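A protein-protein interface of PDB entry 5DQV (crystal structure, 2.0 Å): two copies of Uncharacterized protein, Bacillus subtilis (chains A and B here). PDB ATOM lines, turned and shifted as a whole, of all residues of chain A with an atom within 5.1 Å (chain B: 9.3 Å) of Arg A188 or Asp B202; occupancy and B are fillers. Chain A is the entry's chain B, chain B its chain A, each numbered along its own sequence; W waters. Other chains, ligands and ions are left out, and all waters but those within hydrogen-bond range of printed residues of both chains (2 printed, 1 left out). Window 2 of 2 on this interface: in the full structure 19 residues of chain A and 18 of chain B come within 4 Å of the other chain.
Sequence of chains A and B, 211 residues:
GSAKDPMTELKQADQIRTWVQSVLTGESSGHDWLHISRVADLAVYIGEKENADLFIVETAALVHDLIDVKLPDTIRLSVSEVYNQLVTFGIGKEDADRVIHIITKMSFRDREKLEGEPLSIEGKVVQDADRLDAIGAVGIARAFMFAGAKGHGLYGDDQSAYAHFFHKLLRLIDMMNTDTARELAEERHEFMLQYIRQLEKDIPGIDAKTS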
ATOM      1  N   LEU A  42      29.279 -30.771 -21.391  1.00  0.00           N
ATOM      2  CA  LEU A  42      30.244 -29.669 -21.320  1.00  0.00           C
ATOM      3  C   LEU A  42      31.549 -30.069 -22.024  1.00  0.00           C
ATOM      4  O   LEU A  42      32.185 -29.257 -22.692  1.00  0.00           O
ATOM      5  CB  LEU A  42      30.524 -29.352 -19.839  1.00  0.00           C
ATOM      6  CG  LEU A  42      30.671 -27.966 -19.198  1.00  0.00           C
ATOM      7  CD1 LEU A  42      29.907 -26.834 -19.873  1.00  0.00           C
ATOM      8  CD2 LEU A  42      30.320 -28.064 -17.688  1.00  0.00           C
ATOM      9  N   LEU A 132      34.637 -27.375 -14.034  1.00  0.00           N
ATOM     10  CA  LEU A 132      33.585 -26.372 -14.258  1.00  0.00           C
ATOM     11  C   LEU A 132      32.317 -26.749 -13.525  1.00  0.00           C
ATOM     12  O   LEU A 132      31.659 -25.886 -12.965  1.00  0.00           O
ATOM     13  CB  LEU A 132      33.275 -26.155 -15.738  1.00  0.00           C
ATOM     14  CG  LEU A 132      34.279 -25.254 -16.482  1.00  0.00           C
ATOM     15  CD1 LEU A 132      34.097 -25.353 -17.984  1.00  0.00           C
ATOM     16  CD2 LEU A 132      34.158 -23.816 -16.030  1.00  0.00           C
ATOM     17  N   ASP A 133      32.008 -28.039 -13.495  1.00  0.00           N
ATOM     18  CA  ASP A 133      30.808 -28.522 -12.817  1.00  0.00           C
ATOM     19  C   ASP A 133      30.895 -28.361 -11.299  1.00  0.00           C
ATOM     20  O   ASP A 133      29.890 -28.519 -10.616  1.00  0.00           O
ATOM     21  CB  ASP A 133      30.518 -29.983 -13.169  1.00  0.00           C
ATOM     22  CG  ASP A 133      29.059 -30.385 -12.856  1.00  0.00           C
ATOM     23  OD1 ASP A 133      28.140 -29.761 -13.405  1.00  0.00           O
ATOM     24  OD2 ASP A 133      28.837 -31.304 -12.044  1.00  0.00           O
ATOM     25  N   ILE A 135      32.096 -25.448  -9.918  1.00  0.00           N
ATOM     26  CA  ILE A 135      31.990 -24.033  -9.605  1.00  0.00           C
ATOM     27  C   ILE A 135      30.703 -23.467 -10.159  1.00  0.00           C
ATOM     28  O   ILE A 135      29.929 -24.163 -10.789  1.00  0.00           O
ATOM     29  CB  ILE A 135      33.218 -23.202 -10.042  1.00  0.00           C
ATOM     30  CG1 ILE A 135      33.453 -23.296 -11.552  1.00  0.00           C
ATOM     31  CG2 ILE A 135      34.430 -23.655  -9.263  1.00  0.00           C
ATOM     32  CD1 ILE A 135      34.523 -22.310 -12.097  1.00  0.00           C
ATOM     33  N   GLY A 136      30.487 -22.184  -9.914  1.00  0.00           N
ATOM     34  CA  GLY A 136      29.254 -21.519 -10.314  1.00  0.00           C
ATOM     35  C   GLY A 136      28.100 -21.903  -9.419  1.00  0.00           C
ATOM     36  O   GLY A 136      28.296 -22.435  -8.322  1.00  0.00           O
ATOM     37  N   ALA A 137      26.906 -21.605  -9.901  1.00  0.00           N
ATOM     38  CA  ALA A 137      25.677 -21.936  -9.233  1.00  0.00           C
ATOM     39  C   ALA A 137      25.559 -23.430  -9.062  1.00  0.00           C
ATOM     40  O   ALA A 137      25.126 -23.902  -7.993  1.00  0.00           O
ATOM     41  CB  ALA A 137      24.471 -21.354 -10.037  1.00  0.00           C
ATOM     42  N   VAL A 138      25.982 -24.208 -10.054  1.00  0.00           N
ATOM     43  CA  VAL A 138      25.903 -25.665  -9.926  1.00  0.00           C
ATOM     44  C   VAL A 138      26.919 -26.144  -8.878  1.00  0.00           C
ATOM     45  O   VAL A 138      26.596 -26.973  -8.008  1.00  0.00           O
ATOM     46  CB  VAL A 138      26.071 -26.406 -11.281  1.00  0.00           C
ATOM     47  CG1 VAL A 138      27.454 -26.185 -11.864  1.00  0.00           C
ATOM     48  CG2 VAL A 138      25.815 -27.904 -11.087  1.00  0.00           C
ATOM     49  N   LEU A 184      34.501 -19.890 -19.935  1.00  0.00           N
ATOM     50  CA  LEU A 184      33.313 -20.345 -19.206  1.00  0.00           C
ATOM     51  C   LEU A 184      33.464 -20.130 -17.707  1.00  0.00           C
ATOM     52  O   LEU A 184      32.518 -19.731 -17.030  1.00  0.00           O
ATOM     53  CB  LEU A 184      33.061 -21.829 -19.473  1.00  0.00           C
ATOM     54  CG  LEU A 184      32.555 -22.162 -20.879  1.00  0.00           C
ATOM     55  CD1 LEU A 184      32.557 -23.671 -21.087  1.00  0.00           C
ATOM     56  CD2 LEU A 184      31.160 -21.581 -21.081  1.00  0.00           C
ATOM     57  N   ALA A 185      34.655 -20.382 -17.187  1.00  0.00           N
ATOM     58  CA  ALA A 185      34.909 -20.223 -15.750  1.00  0.00           C
ATOM     59  C   ALA A 185      34.656 -18.804 -15.231  1.00  0.00           C
ATOM     60  O   ALA A 185      34.101 -18.625 -14.141  1.00  0.00           O
ATOM     61  CB  ALA A 185      36.333 -20.655 -15.403  1.00  0.00           C
ATOM     62  N   GLU A 186      35.086 -17.804 -15.990  1.00  0.00           N
ATOM     63  CA  GLU A 186      35.003 -16.414 -15.537  1.00  0.00           C
ATOM     64  C   GLU A 186      33.608 -16.101 -15.003  1.00  0.00           C
ATOM     65  O   GLU A 186      33.474 -15.613 -13.893  1.00  0.00           O
ATOM     66  CB  GLU A 186      35.391 -15.438 -16.643  1.00  0.00           C
ATOM     67  CG  GLU A 186      36.926 -15.350 -16.885  1.00  0.00           C
ATOM     68  CD  GLU A 186      37.341 -14.206 -17.816  1.00  0.00           C
ATOM     69  OE1 GLU A 186      37.436 -13.046 -17.342  1.00  0.00           O
ATOM     70  OE2 GLU A 186      37.599 -14.470 -19.015  1.00  0.00           O
ATOM     71  N   GLU A 187      32.571 -16.411 -15.774  1.00  0.00           N
ATOM     72  CA  GLU A 187      31.184 -16.142 -15.349  1.00  0.00           C
ATOM     73  C   GLU A 187      30.778 -16.940 -14.098  1.00  0.00           C
ATOM     74  O   GLU A 187      30.096 -16.420 -13.198  1.00  0.00           O
ATOM     75  CB  GLU A 187      30.207 -16.485 -16.481  1.00  0.00           C
ATOM     76  CG  GLU A 187      28.803 -15.855 -16.307  1.00  0.00           C
ATOM     77  CD  GLU A 187      28.581 -14.597 -17.151  1.00  0.00           C
ATOM     78  OE1 GLU A 187      29.299 -14.392 -18.162  1.00  0.00           O
ATOM     79  OE2 GLU A 187      27.668 -13.819 -16.803  1.00  0.00           O
ATOM     80  N   ARG A 188      31.160 -18.216 -14.067  1.00  0.00           N
ATOM     81  CA  ARG A 188      30.810 -19.083 -12.940  1.00  0.00           C
ATOM     82  C   ARG A 188      31.562 -18.649 -11.677  1.00  0.00           C
ATOM     83  O   ARG A 188      30.965 -18.523 -10.593  1.00  0.00           O
ATOM     84  CB  ARG A 188      31.093 -20.551 -13.268  1.00  0.00           C
ATOM     85  CG  ARG A 188      30.211 -21.119 -14.364  1.00  0.00           C
ATOM     86  CD  ARG A 188      30.614 -22.569 -14.637  1.00  0.00           C
ATOM     87  NE  ARG A 188      29.793 -23.190 -15.651  1.00  0.00           N
ATOM     88  CZ  ARG A 188      29.176 -24.361 -15.531  1.00  0.00           C
ATOM     89  NH1 ARG A 188      29.219 -25.081 -14.383  1.00  0.00           N
ATOM     90  NH2 ARG A 188      28.446 -24.787 -16.554  1.00  0.00           N
ATOM     91  N   HIS A 189      32.854 -18.372 -11.815  1.00  0.00           N
ATOM     92  CA  HIS A 189      33.641 -17.817 -10.702  1.00  0.00           C
ATOM     93  C   HIS A 189      33.049 -16.511 -10.133  1.00  0.00           C
ATOM     94  O   HIS A 189      32.779 -16.413  -8.926  1.00  0.00           O
ATOM     95  CB  HIS A 189      35.093 -17.620 -11.112  1.00  0.00           C
ATOM     96  CG  HIS A 189      35.987 -17.161  -9.994  1.00  0.00           C
ATOM     97  ND1 HIS A 189      36.523 -18.026  -9.066  1.00  0.00           N
ATOM     98  CD2 HIS A 189      36.427 -15.929  -9.656  1.00  0.00           C
ATOM     99  CE1 HIS A 189      37.260 -17.345  -8.207  1.00  0.00           C
ATOM    100  NE2 HIS A 189      37.230 -16.069  -8.548  1.00  0.00           N
ATOM    101  N   GLU A 190      32.855 -15.512 -10.991  1.00  0.00           N
ATOM    102  CA  GLU A 190      32.204 -14.256 -10.570  1.00  0.00           C
ATOM    103  C   GLU A 190      30.885 -14.476  -9.802  1.00  0.00           C
ATOM    104  O   GLU A 190      30.623 -13.841  -8.763  1.00  0.00           O
ATOM    105  CB  GLU A 190      31.918 -13.396 -11.797  1.00  0.00           C
ATOM    106  CG  GLU A 190      31.122 -12.118 -11.489  1.00  0.00           C
ATOM    107  CD  GLU A 190      31.866 -11.140 -10.594  1.00  0.00           C
ATOM    108  OE1 GLU A 190      33.118 -11.083 -10.676  1.00  0.00           O
ATOM    109  OE2 GLU A 190      31.188 -10.406  -9.835  1.00  0.00           O
ATOM    110  N   PHE A 191      30.042 -15.375 -10.303  1.00  0.00           N
ATOM    111  CA  PHE A 191      28.786 -15.618  -9.630  1.00  0.00           C
ATOM    112  C   PHE A 191      29.002 -16.215  -8.221  1.00  0.00           C
ATOM    113  O   PHE A 191      28.374 -15.781  -7.279  1.00  0.00           O
ATOM    114  CB  PHE A 191      27.833 -16.492 -10.447  1.00  0.00           C
ATOM    115  CG  PHE A 191      26.524 -16.706  -9.753  1.00  0.00           C
ATOM    116  CD1 PHE A 191      25.585 -15.714  -9.735  1.00  0.00           C
ATOM    117  CD2 PHE A 191      26.273 -17.889  -9.054  1.00  0.00           C
ATOM    118  CE1 PHE A 191      24.372 -15.887  -9.072  1.00  0.00           C
ATOM    119  CE2 PHE A 191      25.082 -18.080  -8.388  1.00  0.00           C
ATOM    120  CZ  PHE A 191      24.118 -17.081  -8.384  1.00  0.00           C
ATOM    121  N   MET A 192      29.904 -17.189  -8.083  1.00  0.00           N
ATOM    122  CA  MET A 192      30.189 -17.805  -6.762  1.00  0.00           C
ATOM    123  C   MET A 192      30.618 -16.722  -5.783  1.00  0.00           C
ATOM    124  O   MET A 192      30.360 -16.823  -4.582  1.00  0.00           O
ATOM    125  CB  MET A 192      31.333 -18.816  -6.798  1.00  0.00           C
ATOM    126  CG  MET A 192      31.034 -20.265  -7.046  1.00  0.00           C
ATOM    127  SD  MET A 192      32.423 -21.441  -6.664  1.00  0.00           S
ATOM    128  CE  MET A 192      33.839 -20.538  -7.320  1.00  0.00           C
ATOM    129  N   TYR B 155      18.018 -31.478  -9.247  1.00  0.00           N
ATOM    130  CA  TYR B 155      16.838 -31.192 -10.066  1.00  0.00           C
ATOM    131  C   TYR B 155      16.439 -32.527 -10.680  1.00  0.00           C
ATOM    132  O   TYR B 155      17.106 -33.544 -10.457  1.00  0.00           O
ATOM    133  CB  TYR B 155      17.141 -30.189 -11.183  1.00  0.00           C
ATOM    134  CG  TYR B 155      18.348 -30.595 -12.025  1.00  0.00           C
ATOM    135  CD1 TYR B 155      18.221 -31.428 -13.117  1.00  0.00           C
ATOM    136  CD2 TYR B 155      19.625 -30.163 -11.674  1.00  0.00           C
ATOM    137  CE1 TYR B 155      19.349 -31.791 -13.878  1.00  0.00           C
ATOM    138  CE2 TYR B 155      20.745 -30.504 -12.412  1.00  0.00           C
ATOM    139  CZ  TYR B 155      20.625 -31.329 -13.478  1.00  0.00           C
ATOM    140  OH  TYR B 155      21.768 -31.644 -14.153  1.00  0.00           O
ATOM    141  N   GLN B 194      17.756 -14.693  -8.984  1.00  0.00           N
ATOM    142  CA  GLN B 194      19.024 -14.647  -9.715  1.00  0.00           C
ATOM    143  C   GLN B 194      19.767 -15.985  -9.745  1.00  0.00           C
ATOM    144  O   GLN B 194      20.351 -16.365 -10.784  1.00  0.00           O
ATOM    145  CB  GLN B 194      19.877 -13.465  -9.223  1.00  0.00           C
ATOM    146  CG  GLN B 194      19.211 -12.109  -9.546  1.00  0.00           C
ATOM    147  CD  GLN B 194      18.876 -11.919 -11.081  1.00  0.00           C
ATOM    148  OE1 GLN B 194      19.747 -12.089 -11.947  1.00  0.00           O
ATOM    149  NE2 GLN B 194      17.579 -11.609 -11.394  1.00  0.00           N
ATOM    150  N   TYR B 195      19.697 -16.725  -8.638  1.00  0.00           N
ATOM    151  CA  TYR B 195      20.353 -18.038  -8.494  1.00  0.00           C
ATOM    152  C   TYR B 195      19.713 -19.053  -9.464  1.00  0.00           C
ATOM    153  O   TYR B 195      20.394 -19.748 -10.220  1.00  0.00           O
ATOM    154  CB  TYR B 195      20.294 -18.527  -7.037  1.00  0.00           C
ATOM    155  CG  TYR B 195      21.003 -19.837  -6.908  1.00  0.00           C
ATOM    156  CD1 TYR B 195      20.328 -21.009  -7.188  1.00  0.00           C
ATOM    157  CD2 TYR B 195      22.346 -19.907  -6.618  1.00  0.00           C
ATOM    158  CE1 TYR B 195      20.962 -22.218  -7.125  1.00  0.00           C
ATOM    159  CE2 TYR B 195      23.000 -21.127  -6.575  1.00  0.00           C
ATOM    160  CZ  TYR B 195      22.262 -22.280  -6.849  1.00  0.00           C
ATOM    161  OH  TYR B 195      22.815 -23.541  -6.844  1.00  0.00           O
ATOM    162  N   ILE B 196      18.389 -19.066  -9.499  1.00  0.00           N
ATOM    163  CA  ILE B 196      17.651 -19.869 -10.456  1.00  0.00           C
ATOM    164  C   ILE B 196      18.016 -19.535 -11.904  1.00  0.00           C
ATOM    165  O   ILE B 196      18.216 -20.434 -12.734  1.00  0.00           O
ATOM    166  CB  ILE B 196      16.131 -19.738 -10.226  1.00  0.00           C
ATOM    167  CG1 ILE B 196      15.759 -20.439  -8.922  1.00  0.00           C
ATOM    168  CG2 ILE B 196      15.326 -20.297 -11.406  1.00  0.00           C
ATOM    169  CD1 ILE B 196      14.398 -19.979  -8.399  1.00  0.00           C
ATOM    170  N   ARG B 197      18.079 -18.246 -12.209  1.00  0.00           N
ATOM    171  CA  ARG B 197      18.443 -17.817 -13.544  1.00  0.00           C
ATOM    172  C   ARG B 197      19.818 -18.376 -13.914  1.00  0.00           C
ATOM    173  O   ARG B 197      20.053 -18.886 -15.058  1.00  0.00           O
ATOM    174  CB  ARG B 197      18.472 -16.289 -13.531  1.00  0.00           C
ATOM    175  CG  ARG B 197      18.885 -15.691 -14.835  1.00  0.00           C
ATOM    176  CD  ARG B 197      18.800 -14.212 -14.744  1.00  0.00           C
ATOM    177  NE  ARG B 197      19.317 -13.602 -15.953  1.00  0.00           N
ATOM    178  CZ  ARG B 197      19.962 -12.438 -16.016  1.00  0.00           C
ATOM    179  NH1 ARG B 197      20.195 -11.696 -14.927  1.00  0.00           N
ATOM    180  NH2 ARG B 197      20.344 -12.001 -17.195  1.00  0.00           N
ATOM    181  N   GLN B 198      20.741 -18.275 -12.945  1.00  0.00           N
ATOM    182  CA  GLN B 198      22.097 -18.797 -13.160  1.00  0.00           C
ATOM    183  C   GLN B 198      22.087 -20.317 -13.421  1.00  0.00           C
ATOM    184  O   GLN B 198      22.773 -20.799 -14.362  1.00  0.00           O
ATOM    185  CB  GLN B 198      23.045 -18.366 -12.020  1.00  0.00           C
ATOM    186  CG  GLN B 198      24.518 -18.500 -12.397  1.00  0.00           C
ATOM    187  CD  GLN B 198      24.951 -17.498 -13.421  1.00  0.00           C
ATOM    188  OE1 GLN B 198      24.575 -16.334 -13.371  1.00  0.00           O
ATOM    189  NE2 GLN B 198      25.679 -17.970 -14.421  1.00  0.00           N
ATOM    190  N   LEU B 199      21.272 -21.083 -12.676  1.00  0.00           N
ATOM    191  CA  LEU B 199      21.140 -22.536 -12.928  1.00  0.00           C
ATOM    192  C   LEU B 199      20.561 -22.782 -14.312  1.00  0.00           C
ATOM    193  O   LEU B 199      21.028 -23.684 -15.038  1.00  0.00           O
ATOM    194  CB  LEU B 199      20.260 -23.270 -11.894  1.00  0.00           C
ATOM    195  CG  LEU B 199      20.805 -23.624 -10.531  1.00  0.00           C
ATOM    196  CD1 LEU B 199      19.734 -24.330  -9.728  1.00  0.00           C
ATOM    197  CD2 LEU B 199      22.078 -24.484 -10.687  1.00  0.00           C
ATOM    198  N   GLU B 200      19.568 -21.983 -14.688  1.00  0.00           N
ATOM    199  CA  GLU B 200      18.896 -22.156 -15.995  1.00  0.00           C
ATOM    200  C   GLU B 200      19.897 -21.917 -17.124  1.00  0.00           C
ATOM    201  O   GLU B 200      19.868 -22.619 -18.149  1.00  0.00           O
ATOM    202  CB  GLU B 200      17.683 -21.238 -16.148  1.00  0.00           C
ATOM    203  CG  GLU B 200      16.460 -21.836 -15.475  1.00  0.00           C
ATOM    204  CD  GLU B 200      15.256 -20.929 -15.495  1.00  0.00           C
ATOM    205  OE1 GLU B 200      15.415 -19.709 -15.310  1.00  0.00           O
ATOM    206  OE2 GLU B 200      14.138 -21.445 -15.696  1.00  0.00           O
ATOM    207  N   LYS B 201      20.796 -20.957 -16.902  1.00  0.00           N
ATOM    208  CA  LYS B 201      21.810 -20.590 -17.892  1.00  0.00           C
ATOM    209  C   LYS B 201      22.853 -21.683 -18.016  1.00  0.00           C
ATOM    210  O   LYS B 201      23.153 -22.139 -19.136  1.00  0.00           O
ATOM    211  CB  LYS B 201      22.448 -19.269 -17.485  1.00  0.00           C
ATOM    212  CG  LYS B 201      23.425 -18.650 -18.421  1.00  0.00           C
ATOM    213  CD  LYS B 201      23.765 -17.283 -17.851  1.00  0.00           C
ATOM    214  N   ASP B 202      23.329 -22.166 -16.883  1.00  0.00           N
ATOM    215  CA  ASP B 202      24.420 -23.150 -16.836  1.00  0.00           C
ATOM    216  C   ASP B 202      24.001 -24.570 -17.155  1.00  0.00           C
ATOM    217  O   ASP B 202      24.838 -25.402 -17.558  1.00  0.00           O
ATOM    218  CB  ASP B 202      25.049 -23.109 -15.480  1.00  0.00           C
ATOM    219  CG  ASP B 202      25.840 -21.836 -15.255  1.00  0.00           C
ATOM    220  OD1 ASP B 202      26.015 -21.059 -16.238  1.00  0.00           O
ATOM    221  OD2 ASP B 202      26.270 -21.635 -14.120  1.00  0.00           O
ATOM    222  N   ILE B 203      22.721 -24.847 -16.956  1.00  0.00           N
ATOM    223  CA  ILE B 203      22.134 -26.148 -17.252  1.00  0.00           C
ATOM    224  C   ILE B 203      20.980 -25.993 -18.224  1.00  0.00           C
ATOM    225  O   ILE B 203      19.811 -25.947 -17.813  1.00  0.00           O
ATOM    226  CB  ILE B 203      21.666 -26.890 -15.972  1.00  0.00           C
ATOM    227  CG1 ILE B 203      22.826 -26.998 -14.965  1.00  0.00           C
ATOM    228  CG2 ILE B 203      21.197 -28.320 -16.324  1.00  0.00           C
ATOM    229  CD1 ILE B 203      22.410 -27.535 -13.600  1.00  0.00           C
ATOM    230  N   PRO B 204      21.290 -25.913 -19.535  1.00  0.00           N
ATOM    231  CA  PRO B 204      20.212 -25.829 -20.506  1.00  0.00           C
ATOM    232  C   PRO B 204      19.223 -26.983 -20.327  1.00  0.00           C
ATOM    233  O   PRO B 204      19.637 -28.093 -20.078  1.00  0.00           O
ATOM    234  CB  PRO B 204      20.923 -25.927 -21.850  1.00  0.00           C
ATOM    235  CG  PRO B 204      22.337 -25.482 -21.577  1.00  0.00           C
ATOM    236  CD  PRO B 204      22.632 -25.850 -20.158  1.00  0.00           C
ATOM    237  N   GLY B 205      17.926 -26.711 -20.374  1.00  0.00           N
ATOM    238  CA  GLY B 205      16.966 -27.784 -20.220  1.00  0.00           C
ATOM    239  C   GLY B 205      16.708 -28.214 -18.786  1.00  0.00           C
ATOM    240  O   GLY B 205      15.954 -29.148 -18.573  1.00  0.00           O
ATOM    241  N   ILE B 206      17.285 -27.531 -17.797  1.00  0.00           N
ATOM    242  CA  ILE B 206      17.059 -27.879 -16.382  1.00  0.00           C
ATOM    243  C   ILE B 206      15.558 -27.963 -15.996  1.00  0.00           C
ATOM    244  O   ILE B 206      15.177 -28.844 -15.227  1.00  0.00           O
ATOM    245  CB  ILE B 206      17.796 -26.940 -15.395  1.00  0.00           C
ATOM    246  CG1 ILE B 206      17.796 -27.527 -13.970  1.00  0.00           C
ATOM    247  CG2 ILE B 206      17.170 -25.492 -15.376  1.00  0.00           C
ATOM    248  CD1 ILE B 206      18.607 -26.710 -12.900  1.00  0.00           C
ATOM    249  N   LYS B 209      14.237 -31.361 -17.394  1.00  0.00           N
ATOM    250  CA  LYS B 209      15.070 -32.546 -17.141  1.00  0.00           C
ATOM    251  C   LYS B 209      14.404 -33.512 -16.133  1.00  0.00           C
ATOM    252  O   LYS B 209      13.748 -33.080 -15.177  1.00  0.00           O
ATOM    253  CB  LYS B 209      16.471 -32.137 -16.702  1.00  0.00           C
ATOM    254  CG  LYS B 209      17.470 -31.994 -17.871  1.00  0.00           C
ATOM    255  CD  LYS B 209      18.905 -31.805 -17.384  1.00  0.00           C
ATOM    256  CE  LYS B 209      19.832 -31.245 -18.489  1.00  0.00           C
ATOM    257  NZ  LYS B 209      19.780 -32.073 -19.749  1.00  0.00           N
HETATM  258  O   HOH W   1      27.378 -20.043 -12.337  1.00  0.00           O
HETATM  259  O   HOH W   2      26.585 -27.171 -16.914  1.00  0.00           O
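The guanidinium group (NH1) of Arg A188 sits at hydrogen-bond distance from the backbone carbonyl oxygen (O) of Leu A132, 2.9 Å away.
Water W2 bridges O of Asp B202 (2.6 Å) and NH2 of Arg A188 (3.0 Å).
Water W1 lies within hydrogen-bond range of the side-chain carboxylate (OD2) of Asp B202 (2.6 Å), the backbone NH (N) of Ala A137 (2.9 Å) and the side-chain amide nitrogen (NE2) of Gln B198 (3.4 Å).
Of chain B, only Asp B202 (3.8 Å) comes within 4 Å of Arg A188.
Of chain A, only Arg A188 comes within 4 Å of Asp B202.
Of the printed residues of chain A, Gln B198 touches Ala A137 and Phe A191.
Of the printed residues of chain A, Tyr B195 touches Ala A137 (2.6 Å) and Phe A191 (3.7 Å).
Printed residues of chain B within 4 Å of Phe A191: Tyr B195 (3.7 Å) and Gln B198 (3.8 Å).
Of the printed residues of chain A, Leu B199 touches Ala A137 and Val A138.
Printed residues of chain B within 4 Å of Ala A137: Tyr B195, Gln B198 and Leu B199.
Tyr B155 touches none of the printed residues of chain A.
The nearest residue of chain B that does not touch Arg A188 is Gln B198 (5.5 Å).
The nearest printed residue of chain A that does not touch Asp B202 is Ala A137 (4.3 Å).
The backbone carbonyl oxygen (O) of Ala A137 lies within hydrogen-bond range of the side-chain hydroxyl (OH) of Tyr B195, at 2.6 Å.
Printed residues of chain A that touch a printed residue of chain B: Ala A137, Val A138, Arg A188 and Phe A191.
Hydrophobic or aromatic side chains of chain A that line the printed part of chain B: Ala A137 and Phe A191.
Of the 15 printed residues of chain B, 4 touch a printed residue of chain A.
Hydrophobic or aromatic side chains of chain B within 4 Å of the printed part of chain A: Tyr B195 and Leu B199.
Along chain B the printed residues that touch a printed residue of chain A span positions 195 to 202.
Among the printed residues, no Asp or Glu carboxylate lies within 4 Å of a Lys or Arg side-chain nitrogen of the other chain.
Among the printed residues, pairs that only touch across the chains: Ala A137 with Gln B198, Phe A191 with Tyr B195, Phe A191 with Gln B198, Arg A188 with Asp B202, Val A138 with Leu B199 and Ala A137 with Leu B199.
No position is printed for both chains.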
